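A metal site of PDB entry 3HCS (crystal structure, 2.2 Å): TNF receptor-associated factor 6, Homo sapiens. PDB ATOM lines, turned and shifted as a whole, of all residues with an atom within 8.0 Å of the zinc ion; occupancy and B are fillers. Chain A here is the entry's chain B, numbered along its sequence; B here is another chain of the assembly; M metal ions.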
ATOM      1  N   THR A  34     -25.626  34.374 -13.451  1.00  0.00           N
ATOM      2  CA  THR A  34     -25.217  34.016 -12.102  1.00  0.00           C
ATOM      3  C   THR A  34     -23.850  34.607 -11.776  1.00  0.00           C
ATOM      4  O   THR A  34     -23.106  35.022 -12.667  1.00  0.00           O
ATOM      5  CB  THR A  34     -25.107  32.491 -11.961  1.00  0.00           C
ATOM      6  OG1 THR A  34     -24.075  32.005 -12.821  1.00  0.00           O
ATOM      7  CG2 THR A  34     -26.427  31.835 -12.337  1.00  0.00           C
ATOM      8  N   PRO A  35     -23.478  34.646 -10.477  1.00  0.00           N
ATOM      9  CA  PRO A  35     -22.186  35.197 -10.065  1.00  0.00           C
ATOM     10  C   PRO A  35     -21.044  34.397 -10.691  1.00  0.00           C
ATOM     11  O   PRO A  35     -19.970  34.920 -10.977  1.00  0.00           O
ATOM     12  CB  PRO A  35     -22.196  35.038  -8.549  1.00  0.00           C
ATOM     13  CG  PRO A  35     -23.666  34.973  -8.206  1.00  0.00           C
ATOM     14  CD  PRO A  35     -24.232  34.131  -9.325  1.00  0.00           C
ATOM     15  N   CYS A  36     -21.306  33.119 -10.912  1.00  0.00           N
ATOM     16  CA  CYS A  36     -20.317  32.238 -11.488  1.00  0.00           C
ATOM     17  C   CYS A  36     -20.303  32.279 -13.022  1.00  0.00           C
ATOM     18  O   CYS A  36     -19.792  31.357 -13.669  1.00  0.00           O
ATOM     19  CB  CYS A  36     -20.534  30.798 -11.010  1.00  0.00           C
ATOM     20  SG  CYS A  36     -22.192  30.183 -11.288  1.00  0.00           S
ATOM     21  N   GLY A  37     -20.872  33.331 -13.585  1.00  0.00           N
ATOM     22  CA  GLY A  37     -20.857  33.517 -15.033  1.00  0.00           C
ATOM     23  C   GLY A  37     -21.657  32.609 -15.952  1.00  0.00           C
ATOM     24  O   GLY A  37     -21.237  32.375 -17.093  1.00  0.00           O
ATOM     25  N   HIS A  38     -22.803  32.103 -15.502  1.00  0.00           N
ATOM     26  CA  HIS A  38     -23.626  31.258 -16.353  1.00  0.00           C
ATOM     27  C   HIS A  38     -25.008  31.866 -16.596  1.00  0.00           C
ATOM     28  O   HIS A  38     -25.635  32.407 -15.689  1.00  0.00           O
ATOM     29  CB  HIS A  38     -23.753  29.851 -15.776  1.00  0.00           C
ATOM     30  CG  HIS A  38     -22.516  29.015 -15.953  1.00  0.00           C
ATOM     31  ND1 HIS A  38     -21.593  28.828 -14.944  1.00  0.00           N
ATOM     32  CD2 HIS A  38     -22.025  28.381 -17.034  1.00  0.00           C
ATOM     33  CE1 HIS A  38     -20.590  28.111 -15.406  1.00  0.00           C
ATOM     34  NE2 HIS A  38     -20.827  27.819 -16.678  1.00  0.00           N
ATOM     35  N   ARG A  39     -25.460  31.802 -17.849  1.00  0.00           N
ATOM     36  CA  ARG A  39     -26.746  32.346 -18.253  1.00  0.00           C
ATOM     37  C   ARG A  39     -27.853  31.303 -18.207  1.00  0.00           C
ATOM     38  O   ARG A  39     -27.617  30.133 -18.500  1.00  0.00           O
ATOM     39  CB  ARG A  39     -26.677  32.872 -19.683  1.00  0.00           C
ATOM     40  CG  ARG A  39     -25.727  34.025 -19.914  1.00  0.00           C
ATOM     41  CD  ARG A  39     -25.517  34.228 -21.409  1.00  0.00           C
ATOM     42  NE  ARG A  39     -24.867  35.499 -21.709  1.00  0.00           N
ATOM     43  CZ  ARG A  39     -24.427  35.840 -22.913  1.00  0.00           C
ATOM     44  NH1 ARG A  39     -24.565  35.003 -23.937  1.00  0.00           N
ATOM     45  NH2 ARG A  39     -23.860  37.018 -23.107  1.00  0.00           N
ATOM     46  N   PHE A  40     -29.051  31.726 -17.851  1.00  0.00           N
ATOM     47  CA  PHE A  40     -30.217  30.848 -17.787  1.00  0.00           C
ATOM     48  C   PHE A  40     -31.482  31.669 -18.010  1.00  0.00           C
ATOM     49  O   PHE A  40     -31.459  32.895 -17.862  1.00  0.00           O
ATOM     50  CB  PHE A  40     -30.362  30.186 -16.409  1.00  0.00           C
ATOM     51  CG  PHE A  40     -29.241  29.256 -16.034  1.00  0.00           C
ATOM     52  CD1 PHE A  40     -28.166  29.714 -15.283  1.00  0.00           C
ATOM     53  CD2 PHE A  40     -29.283  27.910 -16.415  1.00  0.00           C
ATOM     54  CE1 PHE A  40     -27.147  28.833 -14.909  1.00  0.00           C
ATOM     55  CE2 PHE A  40     -28.264  27.030 -16.041  1.00  0.00           C
ATOM     56  CZ  PHE A  40     -27.194  27.500 -15.285  1.00  0.00           C
ATOM     57  N   ILE A  45     -33.792  28.797 -14.079  1.00  0.00           N
ATOM     58  CA  ILE A  45     -32.868  28.843 -12.954  1.00  0.00           C
ATOM     59  C   ILE A  45     -33.581  28.973 -11.612  1.00  0.00           C
ATOM     60  O   ILE A  45     -33.152  28.388 -10.621  1.00  0.00           O
ATOM     61  CB  ILE A  45     -31.822  29.972 -13.085  1.00  0.00           C
ATOM     62  CG1 ILE A  45     -30.765  29.821 -11.990  1.00  0.00           C
ATOM     63  CG2 ILE A  45     -32.488  31.333 -13.000  1.00  0.00           C
ATOM     64  CD1 ILE A  45     -29.987  28.526 -12.073  1.00  0.00           C
ATOM     65  N   LYS A  55     -27.964  26.341  -5.829  1.00  0.00           N
ATOM     66  CA  LYS A  55     -26.677  26.223  -6.498  1.00  0.00           C
ATOM     67  C   LYS A  55     -26.834  26.244  -8.011  1.00  0.00           C
ATOM     68  O   LYS A  55     -27.886  25.898  -8.547  1.00  0.00           O
ATOM     69  CB  LYS A  55     -25.987  24.919  -6.078  1.00  0.00           C
ATOM     70  CG  LYS A  55     -26.724  23.654  -6.525  1.00  0.00           C
ATOM     71  CD  LYS A  55     -25.956  22.400  -6.150  1.00  0.00           C
ATOM     72  CE  LYS A  55     -26.769  21.135  -6.437  1.00  0.00           C
ATOM     73  NZ  LYS A  55     -27.224  21.052  -7.861  1.00  0.00           N
ATOM     74  N   CYS A  56     -25.771  26.629  -8.710  1.00  0.00           N
ATOM     75  CA  CYS A  56     -25.807  26.649 -10.170  1.00  0.00           C
ATOM     76  C   CYS A  56     -25.763  25.208 -10.646  1.00  0.00           C
ATOM     77  O   CYS A  56     -24.883  24.449 -10.267  1.00  0.00           O
ATOM     78  CB  CYS A  56     -24.607  27.400 -10.761  1.00  0.00           C
ATOM     79  SG  CYS A  56     -24.510  27.233 -12.577  1.00  0.00           S
ATOM     80  N   PRO A  57     -26.712  24.820 -11.493  1.00  0.00           N
ATOM     81  CA  PRO A  57     -26.743  23.442 -11.991  1.00  0.00           C
ATOM     82  C   PRO A  57     -25.537  23.007 -12.817  1.00  0.00           C
ATOM     83  O   PRO A  57     -25.297  21.816 -12.991  1.00  0.00           O
ATOM     84  CB  PRO A  57     -28.052  23.393 -12.779  1.00  0.00           C
ATOM     85  CG  PRO A  57     -28.178  24.788 -13.293  1.00  0.00           C
ATOM     86  CD  PRO A  57     -27.793  25.624 -12.095  1.00  0.00           C
ATOM     87  N   VAL A  58     -24.778  23.967 -13.339  1.00  0.00           N
ATOM     88  CA  VAL A  58     -23.611  23.632 -14.150  1.00  0.00           C
ATOM     89  C   VAL A  58     -22.347  23.299 -13.372  1.00  0.00           C
ATOM     90  O   VAL A  58     -21.586  22.431 -13.767  1.00  0.00           O
ATOM     91  CB  VAL A  58     -23.272  24.767 -15.150  1.00  0.00           C
ATOM     92  CG1 VAL A  58     -22.031  24.394 -15.959  1.00  0.00           C
ATOM     93  CG2 VAL A  58     -24.442  25.039 -16.079  1.00  0.00           C
ATOM     94  N   ASP A  59     -22.129  23.984 -12.243  1.00  0.00           N
ATOM     95  CA  ASP A  59     -20.915  23.751 -11.463  1.00  0.00           C
ATOM     96  C   ASP A  59     -21.133  23.584  -9.963  1.00  0.00           C
ATOM     97  O   ASP A  59     -20.171  23.546  -9.194  1.00  0.00           O
ATOM     98  CB  ASP A  59     -19.935  24.890 -11.726  1.00  0.00           C
ATOM     99  CG  ASP A  59     -20.623  26.236 -11.696  1.00  0.00           C
ATOM    100  OD1 ASP A  59     -21.483  26.437 -10.808  1.00  0.00           O
ATOM    101  OD2 ASP A  59     -20.297  27.087 -12.550  1.00  0.00           O
ATOM    102  N   ASN A  60     -22.385  23.500  -9.547  1.00  0.00           N
ATOM    103  CA  ASN A  60     -22.711  23.336  -8.131  1.00  0.00           C
ATOM    104  C   ASN A  60     -22.299  24.486  -7.220  1.00  0.00           C
ATOM    105  O   ASN A  60     -22.282  24.326  -6.008  1.00  0.00           O
ATOM    106  CB  ASN A  60     -22.099  22.042  -7.602  1.00  0.00           C
ATOM    107  CG  ASN A  60     -22.598  20.821  -8.316  1.00  0.00           C
ATOM    108  OD1 ASN A  60     -23.802  20.601  -8.431  1.00  0.00           O
ATOM    109  ND2 ASN A  60     -21.671  20.012  -8.815  1.00  0.00           N
ATOM    110  N   GLU A  61     -21.942  25.632  -7.799  1.00  0.00           N
ATOM    111  CA  GLU A  61     -21.559  26.784  -6.997  1.00  0.00           C
ATOM    112  C   GLU A  61     -22.811  27.228  -6.230  1.00  0.00           C
ATOM    113  O   GLU A  61     -23.914  27.166  -6.762  1.00  0.00           O
ATOM    114  CB  GLU A  61     -21.077  27.914  -7.903  1.00  0.00           C
ATOM    115  CG  GLU A  61     -19.840  28.636  -7.397  1.00  0.00           C
ATOM    116  CD  GLU A  61     -18.634  27.725  -7.340  1.00  0.00           C
ATOM    117  OE1 GLU A  61     -18.265  27.179  -8.400  1.00  0.00           O
ATOM    118  OE2 GLU A  61     -18.069  27.554  -6.240  1.00  0.00           O
ATOM    119  N   ILE A  62     -22.649  27.653  -4.987  1.00  0.00           N
ATOM    120  CA  ILE A  62     -23.783  28.104  -4.194  1.00  0.00           C
ATOM    121  C   ILE A  62     -24.435  29.292  -4.889  1.00  0.00           C
ATOM    122  O   ILE A  62     -23.751  30.252  -5.253  1.00  0.00           O
ATOM    123  CB  ILE A  62     -23.353  28.489  -2.778  1.00  0.00           C
ATOM    124  CG1 ILE A  62     -22.958  27.228  -2.017  1.00  0.00           C
ATOM    125  CG2 ILE A  62     -24.485  29.238  -2.072  1.00  0.00           C
ATOM    126  CD1 ILE A  62     -22.389  27.493  -0.650  1.00  0.00           C
ATOM    127  N   LEU A  63     -25.748  29.235  -5.065  1.00  0.00           N
ATOM    128  CA  LEU A  63     -26.480  30.288  -5.736  1.00  0.00           C
ATOM    129  C   LEU A  63     -27.787  30.671  -5.059  1.00  0.00           C
ATOM    130  O   LEU A  63     -28.605  29.811  -4.759  1.00  0.00           O
ATOM    131  CB  LEU A  63     -26.751  29.877  -7.180  1.00  0.00           C
ATOM    132  CG  LEU A  63     -27.644  30.780  -8.041  1.00  0.00           C
ATOM    133  CD1 LEU A  63     -26.973  32.134  -8.270  1.00  0.00           C
ATOM    134  CD2 LEU A  63     -27.913  30.083  -9.356  1.00  0.00           C
ATOM    135  N   ARG B  76     -15.151  35.200 -19.515  1.00  0.00           N
ATOM    136  CA  ARG B  76     -14.715  33.856 -19.876  1.00  0.00           C
ATOM    137  C   ARG B  76     -14.585  33.705 -21.391  1.00  0.00           C
ATOM    138  O   ARG B  76     -13.642  33.113 -21.886  1.00  0.00           O
ATOM    139  CB  ARG B  76     -15.678  32.809 -19.314  1.00  0.00           C
ATOM    140  CG  ARG B  76     -15.258  31.381 -19.611  1.00  0.00           C
ATOM    141  CD  ARG B  76     -16.178  30.393 -18.930  1.00  0.00           C
ATOM    142  NE  ARG B  76     -16.095  30.526 -17.476  1.00  0.00           N
ATOM    143  CZ  ARG B  76     -17.149  30.678 -16.673  1.00  0.00           C
ATOM    144  NH1 ARG B  76     -18.372  30.720 -17.178  1.00  0.00           N
ATOM    145  NH2 ARG B  76     -16.961  30.795 -15.364  1.00  0.00           N
HETATM  146 ZN    ZN M   1     -22.321  28.272 -12.803  1.00  0.00          ZN
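The nearest printed residue that does not touch the zinc ion is Thr 34 (4.1 Å).
The zinc ion is bound by ND1 of His 38 (2.3 Å), OD2 of Asp 59 (2.4 Å), SG of Cys 56 (2.4 Å) and SG of Cys 36 (2.4 Å).
Slightly farther from the zinc ion lies OD1 of Asp 59 (2.8 Å).
N of His 38 is in hydrogen-bond range of OG1 of Thr 34, at 3.0 Å.
N of Glu 61 lies close to OD1 of Asp 59 (3.1 Å).
SG of Cys 56 lies close to N of Val 58 (3.4 Å).
O of Glu 61 lies within hydrogen-bond range of N of Cys 56 (2.7 Å).
The side-chain sulfur (SG) of Cys 36 lies close to the side-chain hydroxyl (OG1) of Thr 34 (3.0 Å).
The backbone carbonyl oxygen of Cys 36 is in hydrogen-bond range of the guanidinium group of Arg 76 of chain B, at 3.3 Å.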
